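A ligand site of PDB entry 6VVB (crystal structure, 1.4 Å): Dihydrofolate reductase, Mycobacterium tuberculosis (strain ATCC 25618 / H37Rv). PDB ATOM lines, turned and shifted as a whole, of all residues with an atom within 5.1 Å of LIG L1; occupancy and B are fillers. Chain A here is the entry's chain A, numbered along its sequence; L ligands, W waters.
The backbone NH (N) of Gln 100 lies within hydrogen-bond range of an oxygen (O9) of LIG L1, at 2.8 Å. An oxygen (O15) of LIG L1 lies within hydrogen-bond range of the side-chain hydroxyl of Ser 68 (2.6 Å). The backbone NH (N) of Gly 98 sits at hydrogen-bond distance from an oxygen (O2) of LIG L1, 3.0 Å away. O4 of LIG L1 is in hydrogen-bond range of N of Arg 46. NE2 of Gln 70 lies within hydrogen-bond range of O15 of LIG L1, 2.8 Å away. The backbone NH of Val 101 sits at hydrogen-bond distance from an oxygen (O1) of LIG L1, 3.3 Å away. N of Gly 99 is in hydrogen-bond range of O9 of LIG L1, 3.1 Å away. The backbone NH (N) of Asp 21 lies within hydrogen-bond range of an oxygen (O12) of LIG L1, 3.5 Å away. N7 of LIG L1 is in hydrogen-bond range of O of Ala 9, at 3.5 Å. An oxygen (O17) of LIG L1 sits at hydrogen-bond distance from the backbone NH (N) of Arg 69 (2.8 Å). O2 of LIG L1 sits at hydrogen-bond distance from N of Thr 48. The backbone carbonyl oxygen (O) of Asp 21 sits at hydrogen-bond distance from an oxygen (O12) of LIG L1 (3.0 Å). The guanidinium group (NH1) of Arg 47 is in salt-bridge range of an oxygen (O8) of LIG L1 (3.1 Å). An oxygen (O3) of LIG L1 sits at hydrogen-bond distance from the backbone NH (N) of Arg 47 (3.4 Å). The guanidinium group (NE) of Arg 46 is in salt-bridge range of an oxygen (O15) of LIG L1 (2.8 Å). OG1 of Thr 48 lies within hydrogen-bond range of O2 of LIG L1 (2.7 Å).
The backbone NH of Gly 45 sits at hydrogen-bond distance from the backbone carbonyl oxygen of Gly 97 (2.8 Å). NE1 of Trp 8 lies within hydrogen-bond range of OE1 of Gln 10, at 2.9 Å. N of Arg 46 sits at hydrogen-bond distance from O of Leu 67, at 3.1 Å. The backbone NH of Gln 70 sits at hydrogen-bond distance from the side-chain hydroxyl of Ser 68 (3.0 Å). The side-chain hydroxyl (OH) of Tyr 102 is in hydrogen-bond range of the backbone carbonyl oxygen (O) of Ile 7, at 2.7 Å. The backbone carbonyl oxygen of Gly 17 is in hydrogen-bond range of the backbone NH of Ala 128 (3.0 Å). The backbone carbonyl oxygen (O) of Thr 48 is in hydrogen-bond range of the side-chain hydroxyl (OG) of Ser 51, at 2.7 Å. The backbone NH of Gly 98 lies within hydrogen-bond range of the side-chain hydroxyl of Thr 48, at 3.1 Å.
O of Ile 16 lies close to O14 of LIG L1, at 3.0 Å. Residues that only touch LIG L1: Trp 8, Gly 17, Arg 18, Gly 20, Ile 22, Trp 24, Gly 45, Leu 67, Gly 82, Ile 96, Gly 97, Tyr 102, Leu 104 and Ala 128.
Water W1 bridges an oxygen (O13) of LIG L1 (2.7 Å) and the side-chain hydroxyl of Ser 51 (2.7 Å). Water W8 bridges O12 of LIG L1 and N of Gly 20. Water W5 bridges an oxygen (O5) of LIG L1 (2.8 Å) and the side-chain amide nitrogen of Gln 100 (3.5 Å). Water W7 lies within hydrogen-bond range of the backbone carbonyl oxygen of Gly 82 and a nitrogen (N4) of LIG L1.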
ATOM      1  N   ILE A   7       9.154   8.292  18.101  1.00  0.00           N
ATOM      2  CA  ILE A   7       8.664   8.178  19.470  1.00  0.00           C
ATOM      3  C   ILE A   7       8.999   6.785  19.977  1.00  0.00           C
ATOM      4  O   ILE A   7       8.670   5.782  19.329  1.00  0.00           O
ATOM      5  CB  ILE A   7       7.151   8.486  19.573  1.00  0.00           C
ATOM      6  CG1 ILE A   7       6.657   8.260  21.005  1.00  0.00           C
ATOM      7  CG2 ILE A   7       6.346   7.675  18.556  1.00  0.00           C
ATOM      8  CD1 ILE A   7       5.328   8.910  21.302  1.00  0.00           C
ATOM      9  N   TRP A   8       9.690   6.718  21.118  1.00  0.00           N
ATOM     10  CA  TRP A   8      10.095   5.438  21.687  1.00  0.00           C
ATOM     11  C   TRP A   8      10.268   5.559  23.189  1.00  0.00           C
ATOM     12  O   TRP A   8      10.331   6.661  23.736  1.00  0.00           O
ATOM     13  CB  TRP A   8      11.391   4.879  21.053  1.00  0.00           C
ATOM     14  CG  TRP A   8      12.704   5.482  21.488  1.00  0.00           C
ATOM     15  CD1 TRP A   8      13.495   5.073  22.539  1.00  0.00           C
ATOM     16  CD2 TRP A   8      13.443   6.505  20.806  1.00  0.00           C
ATOM     17  NE1 TRP A   8      14.644   5.838  22.578  1.00  0.00           N
ATOM     18  CE2 TRP A   8      14.635   6.719  21.530  1.00  0.00           C
ATOM     19  CE3 TRP A   8      13.167   7.295  19.691  1.00  0.00           C
ATOM     20  CZ2 TRP A   8      15.581   7.668  21.146  1.00  0.00           C
ATOM     21  CZ3 TRP A   8      14.115   8.252  19.312  1.00  0.00           C
ATOM     22  CH2 TRP A   8      15.298   8.422  20.037  1.00  0.00           C
ATOM     23  N   ALA A   9      10.355   4.406  23.844  1.00  0.00           N
ATOM     24  CA  ALA A   9      10.691   4.309  25.257  1.00  0.00           C
ATOM     25  C   ALA A   9      11.922   3.424  25.409  1.00  0.00           C
ATOM     26  O   ALA A   9      12.047   2.395  24.731  1.00  0.00           O
ATOM     27  CB  ALA A   9       9.532   3.711  26.048  1.00  0.00           C
ATOM     28  N   GLN A  10      12.840   3.807  26.298  1.00  0.00           N
ATOM     29  CA  GLN A  10      14.060   3.026  26.473  1.00  0.00           C
ATOM     30  C   GLN A  10      14.365   2.866  27.952  1.00  0.00           C
ATOM     31  O   GLN A  10      14.078   3.748  28.759  1.00  0.00           O
ATOM     32  CB  GLN A  10      15.276   3.655  25.775  1.00  0.00           C
ATOM     33  CG  GLN A  10      15.643   5.034  26.326  1.00  0.00           C
ATOM     34  CD  GLN A  10      16.852   5.627  25.635  1.00  0.00           C
ATOM     35  OE1 GLN A  10      16.827   5.891  24.432  1.00  0.00           O
ATOM     36  NE2 GLN A  10      17.936   5.797  26.377  1.00  0.00           N
ATOM     37  N   ILE A  16      15.416  -1.256  23.970  1.00  0.00           N
ATOM     38  CA  ILE A  16      14.016  -0.982  23.674  1.00  0.00           C
ATOM     39  C   ILE A  16      13.198  -2.238  23.448  1.00  0.00           C
ATOM     40  O   ILE A  16      11.959  -2.182  23.525  1.00  0.00           O
ATOM     41  CB  ILE A  16      13.858  -0.024  22.473  1.00  0.00           C
ATOM     42  CG1 ILE A  16      14.334  -0.682  21.181  1.00  0.00           C
ATOM     43  CG2 ILE A  16      14.607   1.288  22.730  1.00  0.00           C
ATOM     44  CD1 ILE A  16      13.886   0.074  19.940  1.00  0.00           C
ATOM     45  N   GLY A  17      13.819  -3.386  23.168  1.00  0.00           N
ATOM     46  CA  GLY A  17      13.057  -4.590  22.886  1.00  0.00           C
ATOM     47  C   GLY A  17      13.879  -5.832  23.099  1.00  0.00           C
ATOM     48  O   GLY A  17      15.113  -5.808  23.003  1.00  0.00           O
ATOM     49  N   ARG A  18      13.193  -6.923  23.407  1.00  0.00           N
ATOM     50  CA  ARG A  18      13.839  -8.205  23.637  1.00  0.00           C
ATOM     51  C   ARG A  18      12.794  -9.285  23.412  1.00  0.00           C
ATOM     52  O   ARG A  18      11.643  -9.130  23.834  1.00  0.00           O
ATOM     53  CB  ARG A  18      14.324  -8.273  25.086  1.00  0.00           C
ATOM     54  CG  ARG A  18      14.948  -9.596  25.471  1.00  0.00           C
ATOM     55  CD  ARG A  18      15.570  -9.519  26.849  1.00  0.00           C
ATOM     56  NE  ARG A  18      16.648  -8.527  26.900  1.00  0.00           N
ATOM     57  CZ  ARG A  18      17.226  -8.097  28.015  1.00  0.00           C
ATOM     58  NH1 ARG A  18      16.856  -8.567  29.201  1.00  0.00           N
ATOM     59  NH2 ARG A  18      18.191  -7.189  27.943  1.00  0.00           N
ATOM     60  N   GLY A  20      10.990 -10.097  20.938  1.00  0.00           N
ATOM     61  CA  GLY A  20       9.801  -9.699  20.227  1.00  0.00           C
ATOM     62  C   GLY A  20       8.807  -8.894  21.034  1.00  0.00           C
ATOM     63  O   GLY A  20       7.663  -8.720  20.602  1.00  0.00           O
ATOM     64  N   ASP A  21       9.205  -8.397  22.206  1.00  0.00           N
ATOM     65  CA  ASP A  21       8.328  -7.638  23.075  1.00  0.00           C
ATOM     66  C   ASP A  21       9.116  -6.477  23.648  1.00  0.00           C
ATOM     67  O   ASP A  21      10.309  -6.307  23.378  1.00  0.00           O
ATOM     68  CB  ASP A  21       7.806  -8.556  24.192  1.00  0.00           C
ATOM     69  CG  ASP A  21       6.435  -8.151  24.734  1.00  0.00           C
ATOM     70  OD1 ASP A  21       5.719  -9.049  25.234  1.00  0.00           O
ATOM     71  OD2 ASP A  21       6.074  -6.955  24.682  1.00  0.00           O
ATOM     72  N   ILE A  22       8.435  -5.645  24.428  1.00  0.00           N
ATOM     73  CA  ILE A  22       9.076  -4.597  25.213  1.00  0.00           C
ATOM     74  C   ILE A  22       9.194  -5.104  26.643  1.00  0.00           C
ATOM     75  O   ILE A  22       8.193  -5.573  27.209  1.00  0.00           O
ATOM     76  CB  ILE A  22       8.263  -3.283  25.167  1.00  0.00           C
ATOM     77  CG1 ILE A  22       8.154  -2.794  23.724  1.00  0.00           C
ATOM     78  CG2 ILE A  22       8.899  -2.223  26.064  1.00  0.00           C
ATOM     79  CD1 ILE A  22       7.190  -1.640  23.540  1.00  0.00           C
ATOM     80  N   TRP A  24       9.139  -4.126  29.635  1.00  0.00           N
ATOM     81  CA  TRP A  24       8.502  -3.453  30.767  1.00  0.00           C
ATOM     82  C   TRP A  24       7.125  -3.008  30.308  1.00  0.00           C
ATOM     83  O   TRP A  24       6.789  -3.075  29.123  1.00  0.00           O
ATOM     84  CB  TRP A  24       9.316  -2.246  31.264  1.00  0.00           C
ATOM     85  CG  TRP A  24       9.435  -1.189  30.201  1.00  0.00           C
ATOM     86  CD1 TRP A  24       8.512  -0.221  29.894  1.00  0.00           C
ATOM     87  CD2 TRP A  24      10.509  -1.029  29.273  1.00  0.00           C
ATOM     88  NE1 TRP A  24       8.961   0.530  28.840  1.00  0.00           N
ATOM     89  CE2 TRP A  24      10.186   0.058  28.444  1.00  0.00           C
ATOM     90  CE3 TRP A  24      11.720  -1.703  29.070  1.00  0.00           C
ATOM     91  CZ2 TRP A  24      11.017   0.482  27.419  1.00  0.00           C
ATOM     92  CZ3 TRP A  24      12.548  -1.274  28.058  1.00  0.00           C
ATOM     93  CH2 TRP A  24      12.198  -0.185  27.238  1.00  0.00           C
ATOM     94  N   GLY A  45       8.287  -0.934  11.599  1.00  0.00           N
ATOM     95  CA  GLY A  45       8.822  -2.134  10.992  1.00  0.00           C
ATOM     96  C   GLY A  45       7.886  -3.313  11.108  1.00  0.00           C
ATOM     97  O   GLY A  45       7.027  -3.385  11.999  1.00  0.00           O
ATOM     98  N   ARG A  46       8.082  -4.294  10.221  1.00  0.00           N
ATOM     99  CA  ARG A  46       7.185  -5.439  10.190  1.00  0.00           C
ATOM    100  C   ARG A  46       7.209  -6.221  11.505  1.00  0.00           C
ATOM    101  O   ARG A  46       6.174  -6.738  11.935  1.00  0.00           O
ATOM    102  CB  ARG A  46       7.522  -6.334   8.992  1.00  0.00           C
ATOM    103  CG  ARG A  46       6.445  -7.357   8.648  1.00  0.00           C
ATOM    104  CD  ARG A  46       6.830  -8.722   9.147  1.00  0.00           C
ATOM    105  NE  ARG A  46       8.243  -9.017   8.905  1.00  0.00           N
ATOM    106  CZ  ARG A  46       8.957  -9.785   9.708  1.00  0.00           C
ATOM    107  NH1 ARG A  46       8.381 -10.339  10.768  1.00  0.00           N
ATOM    108  NH2 ARG A  46      10.243 -10.017   9.443  1.00  0.00           N
ATOM    109  N   ARG A  47       8.372  -6.306  12.154  1.00  0.00           N
ATOM    110  CA  ARG A  47       8.426  -7.036  13.422  1.00  0.00           C
ATOM    111  C   ARG A  47       7.602  -6.347  14.489  1.00  0.00           C
ATOM    112  O   ARG A  47       6.974  -7.001  15.344  1.00  0.00           O
ATOM    113  CB  ARG A  47       9.869  -7.180  13.892  1.00  0.00           C
ATOM    114  CG  ARG A  47      10.699  -8.130  13.079  1.00  0.00           C
ATOM    115  CD  ARG A  47      12.123  -8.153  13.610  1.00  0.00           C
ATOM    116  NE  ARG A  47      12.982  -9.059  12.856  1.00  0.00           N
ATOM    117  CZ  ARG A  47      14.302  -9.104  12.989  1.00  0.00           C
ATOM    118  NH1 ARG A  47      14.924  -8.299  13.851  1.00  0.00           N
ATOM    119  NH2 ARG A  47      15.009  -9.959  12.265  1.00  0.00           N
ATOM    120  N   THR A  48       7.617  -5.008  14.492  1.00  0.00           N
ATOM    121  CA  THR A  48       6.804  -4.279  15.459  1.00  0.00           C
ATOM    122  C   THR A  48       5.314  -4.468  15.184  1.00  0.00           C
ATOM    123  O   THR A  48       4.535  -4.686  16.125  1.00  0.00           O
ATOM    124  CB  THR A  48       7.224  -2.802  15.469  1.00  0.00           C
ATOM    125  OG1 THR A  48       8.553  -2.698  15.996  1.00  0.00           O
ATOM    126  CG2 THR A  48       6.284  -1.964  16.321  1.00  0.00           C
ATOM    127  N   SER A  51       4.182  -7.596  16.610  1.00  0.00           N
ATOM    128  CA  SER A  51       4.168  -7.580  18.061  1.00  0.00           C
ATOM    129  C   SER A  51       2.917  -6.936  18.645  1.00  0.00           C
ATOM    130  O   SER A  51       2.667  -7.084  19.846  1.00  0.00           O
ATOM    131  CB  SER A  51       5.433  -6.888  18.565  1.00  0.00           C
ATOM    132  OG  SER A  51       5.250  -5.488  18.576  1.00  0.00           O
ATOM    133  N   LEU A  67       6.695  -1.166   7.133  1.00  0.00           N
ATOM    134  CA  LEU A  67       7.831  -1.363   6.246  1.00  0.00           C
ATOM    135  C   LEU A  67       8.187  -2.842   6.182  1.00  0.00           C
ATOM    136  O   LEU A  67       8.315  -3.520   7.208  1.00  0.00           O
ATOM    137  CB  LEU A  67       9.052  -0.590   6.744  1.00  0.00           C
ATOM    138  CG  LEU A  67       8.920   0.915   6.996  1.00  0.00           C
ATOM    139  CD1 LEU A  67      10.271   1.495   7.371  1.00  0.00           C
ATOM    140  CD2 LEU A  67       8.390   1.592   5.787  1.00  0.00           C
ATOM    141  N   SER A  68       8.346  -3.339   4.954  1.00  0.00           N
ATOM    142  CA  SER A  68       8.801  -4.701   4.713  1.00  0.00           C
ATOM    143  C   SER A  68       9.465  -4.775   3.346  1.00  0.00           C
ATOM    144  O   SER A  68       9.074  -4.071   2.423  1.00  0.00           O
ATOM    145  CB  SER A  68       7.632  -5.694   4.658  1.00  0.00           C
ATOM    146  OG  SER A  68       8.086  -7.028   4.562  1.00  0.00           O
ATOM    147  N   ARG A  69      10.456  -5.657   3.238  1.00  0.00           N
ATOM    148  CA  ARG A  69      11.036  -5.975   1.933  1.00  0.00           C
ATOM    149  C   ARG A  69      10.317  -7.131   1.255  1.00  0.00           C
ATOM    150  O   ARG A  69      10.672  -7.465   0.119  1.00  0.00           O
ATOM    151  CB  ARG A  69      12.510  -6.350   2.085  1.00  0.00           C
ATOM    152  CG  ARG A  69      13.432  -5.270   2.582  1.00  0.00           C
ATOM    153  CD  ARG A  69      14.840  -5.841   2.631  1.00  0.00           C
ATOM    154  NE  ARG A  69      15.787  -4.958   3.319  1.00  0.00           N
ATOM    155  CZ  ARG A  69      16.047  -5.014   4.619  1.00  0.00           C
ATOM    156  NH1 ARG A  69      15.414  -5.905   5.378  1.00  0.00           N
ATOM    157  NH2 ARG A  69      16.924  -4.189   5.159  1.00  0.00           N
ATOM    158  N   GLN A  70       9.344  -7.746   1.914  1.00  0.00           N
ATOM    159  CA  GLN A  70       8.658  -8.902   1.354  1.00  0.00           C
ATOM    160  C   GLN A  70       7.572  -8.443   0.396  1.00  0.00           C
ATOM    161  O   GLN A  70       6.648  -7.727   0.794  1.00  0.00           O
ATOM    162  CB  GLN A  70       8.024  -9.734   2.464  1.00  0.00           C
ATOM    163  CG  GLN A  70       9.008 -10.331   3.443  1.00  0.00           C
ATOM    164  CD  GLN A  70       8.313 -11.174   4.490  1.00  0.00           C
ATOM    165  OE1 GLN A  70       7.785 -12.251   4.197  1.00  0.00           O
ATOM    166  NE2 GLN A  70       8.288 -10.669   5.713  1.00  0.00           N
ATOM    167  N   GLY A  82       7.792  -0.666   0.739  1.00  0.00           N
ATOM    168  CA  GLY A  82       9.109  -1.251   0.655  1.00  0.00           C
ATOM    169  C   GLY A  82      10.261  -0.320   0.945  1.00  0.00           C
ATOM    170  O   GLY A  82      11.413  -0.747   0.891  1.00  0.00           O
ATOM    171  N   SER A  83       9.974   0.941   1.267  1.00  0.00           N
ATOM    172  CA  SER A  83      10.999   1.913   1.597  1.00  0.00           C
ATOM    173  C   SER A  83      10.372   2.929   2.553  1.00  0.00           C
ATOM    174  O   SER A  83       9.172   3.177   2.509  1.00  0.00           O
ATOM    175  CB  SER A  83      11.504   2.631   0.342  1.00  0.00           C
ATOM    176  OG  SER A  83      10.712   3.758   0.051  1.00  0.00           O
ATOM    177  N   ILE A  96       7.220   4.635  14.949  1.00  0.00           N
ATOM    178  CA  ILE A  96       6.884   4.055  16.246  1.00  0.00           C
ATOM    179  C   ILE A  96       7.668   2.787  16.525  1.00  0.00           C
ATOM    180  O   ILE A  96       7.356   2.084  17.495  1.00  0.00           O
ATOM    181  CB  ILE A  96       5.369   3.823  16.416  1.00  0.00           C
ATOM    182  CG1 ILE A  96       4.888   2.732  15.449  1.00  0.00           C
ATOM    183  CG2 ILE A  96       4.627   5.138  16.228  1.00  0.00           C
ATOM    184  CD1 ILE A  96       3.558   2.079  15.888  1.00  0.00           C
ATOM    185  N   GLY A  97       8.681   2.467  15.726  1.00  0.00           N
ATOM    186  CA  GLY A  97       9.594   1.373  16.014  1.00  0.00           C
ATOM    187  C   GLY A  97       9.693   0.419  14.851  1.00  0.00           C
ATOM    188  O   GLY A  97       9.008   0.561  13.828  1.00  0.00           O
ATOM    189  N   GLY A  98      10.568  -0.585  14.982  1.00  0.00           N
ATOM    190  CA  GLY A  98      11.402  -0.828  16.160  1.00  0.00           C
ATOM    191  C   GLY A  98      12.838  -0.392  15.916  1.00  0.00           C
ATOM    192  O   GLY A  98      13.064   0.632  15.268  1.00  0.00           O
ATOM    193  N   GLY A  99      13.793  -1.174  16.426  1.00  0.00           N
ATOM    194  CA  GLY A  99      15.193  -0.752  16.400  1.00  0.00           C
ATOM    195  C   GLY A  99      15.700  -0.440  14.997  1.00  0.00           C
ATOM    196  O   GLY A  99      16.319   0.593  14.763  1.00  0.00           O
ATOM    197  N   GLN A 100      15.442  -1.348  14.048  1.00  0.00           N
ATOM    198  CA  GLN A 100      15.913  -1.115  12.679  1.00  0.00           C
ATOM    199  C   GLN A 100      15.283   0.118  12.073  1.00  0.00           C
ATOM    200  O   GLN A 100      15.962   0.913  11.412  1.00  0.00           O
ATOM    201  CB  GLN A 100      15.610  -2.327  11.804  1.00  0.00           C
ATOM    202  CG  GLN A 100      16.350  -3.573  12.213  1.00  0.00           C
ATOM    203  CD  GLN A 100      16.145  -4.725  11.247  1.00  0.00           C
ATOM    204  OE1 GLN A 100      15.540  -4.562  10.194  1.00  0.00           O
ATOM    205  NE2 GLN A 100      16.641  -5.898  11.618  1.00  0.00           N
ATOM    206  N   VAL A 101      13.985   0.310  12.266  1.00  0.00           N
ATOM    207  CA  VAL A 101      13.317   1.430  11.605  1.00  0.00           C
ATOM    208  C   VAL A 101      13.676   2.765  12.244  1.00  0.00           C
ATOM    209  O   VAL A 101      13.783   3.778  11.535  1.00  0.00           O
ATOM    210  CB  VAL A 101      11.806   1.187  11.467  1.00  0.00           C
ATOM    211  CG1 VAL A 101      11.135   2.349  10.771  1.00  0.00           C
ATOM    212  CG2 VAL A 101      11.581  -0.060  10.647  1.00  0.00           C
ATOM    213  N   TYR A 102      13.910   2.806  13.567  1.00  0.00           N
ATOM    214  CA  TYR A 102      14.416   4.038  14.164  1.00  0.00           C
ATOM    215  C   TYR A 102      15.748   4.442  13.542  1.00  0.00           C
ATOM    216  O   TYR A 102      15.973   5.620  13.260  1.00  0.00           O
ATOM    217  CB  TYR A 102      14.582   3.906  15.672  1.00  0.00           C
ATOM    218  CG  TYR A 102      13.301   3.797  16.477  1.00  0.00           C
ATOM    219  CD1 TYR A 102      13.170   2.799  17.434  1.00  0.00           C
ATOM    220  CD2 TYR A 102      12.243   4.690  16.306  1.00  0.00           C
ATOM    221  CE1 TYR A 102      12.029   2.674  18.191  1.00  0.00           C
ATOM    222  CE2 TYR A 102      11.088   4.580  17.061  1.00  0.00           C
ATOM    223  CZ  TYR A 102      10.992   3.563  17.994  1.00  0.00           C
ATOM    224  OH  TYR A 102       9.848   3.421  18.743  1.00  0.00           O
ATOM    225  N   LEU A 104      16.883   3.714  10.613  1.00  0.00           N
ATOM    226  CA  LEU A 104      16.637   4.131   9.232  1.00  0.00           C
ATOM    227  C   LEU A 104      16.066   5.544   9.183  1.00  0.00           C
ATOM    228  O   LEU A 104      16.403   6.335   8.274  1.00  0.00           O
ATOM    229  CB  LEU A 104      15.661   3.147   8.596  1.00  0.00           C
ATOM    230  CG  LEU A 104      15.446   3.091   7.096  1.00  0.00           C
ATOM    231  CD1 LEU A 104      16.686   2.539   6.408  1.00  0.00           C
ATOM    232  CD2 LEU A 104      14.255   2.194   6.822  1.00  0.00           C
ATOM    233  N   ALA A 128      17.004  -5.242  20.693  1.00  0.00           N
ATOM    234  CA  ALA A 128      16.822  -4.026  19.911  1.00  0.00           C
ATOM    235  C   ALA A 128      17.212  -2.830  20.781  1.00  0.00           C
ATOM    236  O   ALA A 128      16.860  -2.765  21.971  1.00  0.00           O
ATOM    237  CB  ALA A 128      15.360  -3.895  19.473  1.00  0.00           C
HETATM  238  P1  LIG L   1      11.566  -3.623  13.413  1.00  0.00           P
HETATM  239  O1  LIG L   1      12.410  -2.387  13.181  1.00  0.00           O
HETATM  240  O2  LIG L   1      10.283  -3.450  14.121  1.00  0.00           O
HETATM  241  O3  LIG L   1      11.226  -4.414  11.988  1.00  0.00           O
HETATM  242  C1  LIG L   1      12.328  -4.920  11.202  1.00  0.00           C
HETATM  243  C2  LIG L   1      11.758  -5.359   9.857  1.00  0.00           C
HETATM  244  O4  LIG L   1      11.360  -3.998   9.129  1.00  0.00           O
HETATM  245  C3  LIG L   1      12.628  -5.899   9.034  1.00  0.00           C
HETATM  246  O5  LIG L   1      12.806  -7.347   9.270  1.00  0.00           O
HETATM  247  C4  LIG L   1      11.993  -5.650   7.631  1.00  0.00           C
HETATM  248  O6  LIG L   1      10.852  -6.359   7.461  1.00  0.00           O
HETATM  249  C5  LIG L   1      11.561  -4.198   7.823  1.00  0.00           C
HETATM  250  N1  LIG L   1      12.607  -3.315   7.324  1.00  0.00           N
HETATM  251  C6  LIG L   1      13.633  -3.011   8.122  1.00  0.00           C
HETATM  252  N2  LIG L   1      14.436  -2.217   7.411  1.00  0.00           N
HETATM  253  C7  LIG L   1      13.892  -2.047   6.188  1.00  0.00           C
HETATM  254  C8  LIG L   1      14.287  -1.355   5.091  1.00  0.00           C
HETATM  255  N3  LIG L   1      15.344  -0.469   4.539  1.00  0.00           N
HETATM  256  N4  LIG L   1      13.522  -1.380   4.005  1.00  0.00           N
HETATM  257  C9  LIG L   1      12.375  -2.088   3.966  1.00  0.00           C
HETATM  258  N5  LIG L   1      11.976  -2.774   5.051  1.00  0.00           N
HETATM  259  C10 LIG L   1      12.765  -2.744   6.140  1.00  0.00           C
HETATM  260  O7  LIG L   1      12.455  -4.812  14.113  1.00  0.00           O
HETATM  261  P2  LIG L   1      13.435  -4.719  15.400  1.00  0.00           P
HETATM  262  O8  LIG L   1      13.751  -6.164  15.729  1.00  0.00           O
HETATM  263  O9  LIG L   1      14.625  -3.842  15.140  1.00  0.00           O
HETATM  264  O10 LIG L   1      12.539  -4.064  16.607  1.00  0.00           O
HETATM  265  C11 LIG L   1      11.472  -4.847  17.121  1.00  0.00           C
HETATM  266  C12 LIG L   1      11.611  -4.881  18.714  1.00  0.00           C
HETATM  267  O11 LIG L   1      11.440  -3.410  19.113  1.00  0.00           O
HETATM  268  C13 LIG L   1      10.671  -5.536  19.304  1.00  0.00           C
HETATM  269  O12 LIG L   1      11.206  -6.124  20.539  1.00  0.00           O
HETATM  270  C14 LIG L   1       9.574  -4.413  19.787  1.00  0.00           C
HETATM  271  O13 LIG L   1       8.765  -4.937  20.907  1.00  0.00           O
HETATM  272  C15 LIG L   1      10.354  -3.459  20.188  1.00  0.00           C
HETATM  273  N6  LIG L   1       9.756  -2.117  20.131  1.00  0.00           N
HETATM  274  C16 LIG L   1      10.072  -1.302  21.211  1.00  0.00           C
HETATM  275  C17 LIG L   1       9.501   0.041  21.316  1.00  0.00           C
HETATM  276  C18 LIG L   1       9.879   0.832  22.506  1.00  0.00           C
HETATM  277  O14 LIG L   1      10.440   0.409  23.480  1.00  0.00           O
HETATM  278  N7  LIG L   1       9.494   2.179  22.416  1.00  0.00           N
HETATM  279  C19 LIG L   1       8.464   0.603  20.318  1.00  0.00           C
HETATM  280  C20 LIG L   1       8.354  -0.270  19.041  1.00  0.00           C
HETATM  281  C21 LIG L   1       8.982  -1.670  19.020  1.00  0.00           C
HETATM  282  P3  LIG L   1      10.828  -7.747   6.542  1.00  0.00           P
HETATM  283  O15 LIG L   1       9.389  -8.159   6.477  1.00  0.00           O
HETATM  284  O16 LIG L   1      11.673  -8.733   7.311  1.00  0.00           O
HETATM  285  O17 LIG L   1      11.457  -7.440   5.208  1.00  0.00           O
HETATM  286  C1  LG2 L   2      -3.198  -1.990  24.207  1.00  0.00           C
HETATM  287  C2  LG2 L   2       4.935   0.229  19.635  1.00  0.00           C
HETATM  288  C3  LG2 L   2       4.898  -1.024  20.203  1.00  0.00           C
HETATM  289  C4  LG2 L   2       3.821   1.036  19.739  1.00  0.00           C
HETATM  290  C5  LG2 L   2       3.775  -1.521  20.897  1.00  0.00           C
HETATM  291  C6  LG2 L   2       2.675   0.617  20.401  1.00  0.00           C
HETATM  292  C7  LG2 L   2       1.372  -2.322  22.219  1.00  0.00           C
HETATM  293  C8  LG2 L   2      -2.026   1.089  22.088  1.00  0.00           C
HETATM  294  C9  LG2 L   2      -3.257   3.201  21.543  1.00  0.00           C
HETATM  295  C10 LG2 L   2      -3.010  -0.680  23.443  1.00  0.00           C
HETATM  296  C11 LG2 L   2       2.653  -0.662  20.992  1.00  0.00           C
HETATM  297  C12 LG2 L   2       1.487  -1.092  21.663  1.00  0.00           C
HETATM  298  C13 LG2 L   2      -3.187   1.826  22.235  1.00  0.00           C
HETATM  299  C14 LG2 L   2      -1.898  -0.200  22.700  1.00  0.00           C
HETATM  300  C15 LG2 L   2      -0.680  -0.910  22.499  1.00  0.00           C
HETATM  301  C16 LG2 L   2      -4.229   1.278  22.991  1.00  0.00           C
HETATM  302  C17 LG2 L   2      -5.570   1.949  23.253  1.00  0.00           C
HETATM  303  F1  LG2 L   2      -6.096   1.233  24.448  1.00  0.00           F
HETATM  304  F2  LG2 L   2      -5.402   3.362  23.556  1.00  0.00           F
HETATM  305  F3  LG2 L   2      -6.399   1.650  22.034  1.00  0.00           F
HETATM  306  N1  LG2 L   2      -4.089   0.074  23.547  1.00  0.00           N
HETATM  307  N2  LG2 L   2       0.338  -0.341  21.823  1.00  0.00           N
HETATM  308  O1  LG2 L   2      -2.302   4.004  21.412  1.00  0.00           O
HETATM  309  O2  LG2 L   2      -4.360   3.553  21.083  1.00  0.00           O
HETATM  310  S1  LG2 L   2      -0.186  -2.502  22.946  1.00  0.00           S
HETATM  311  O   HOH W   1       6.227  -4.174  20.783  1.00  0.00           O
HETATM  312  O   HOH W   2      17.180  -1.338   7.646  1.00  0.00           O
HETATM  313  O   HOH W   3      17.081  -4.403  16.078  1.00  0.00           O
HETATM  314  O   HOH W   4       7.099   3.563  22.364  1.00  0.00           O
HETATM  315  O   HOH W   5      15.530  -8.154   9.204  1.00  0.00           O
HETATM  316  O   HOH W   6      12.547  -8.190  17.295  1.00  0.00           O
HETATM  317  O   HOH W   7      14.122  -0.344   1.393  1.00  0.00           O
HETATM  318  O   HOH W   8      12.892  -8.186  19.962  1.00  0.00           O
HETATM  319  O   HOH W   9      15.943  -6.879  17.467  1.00  0.00           O
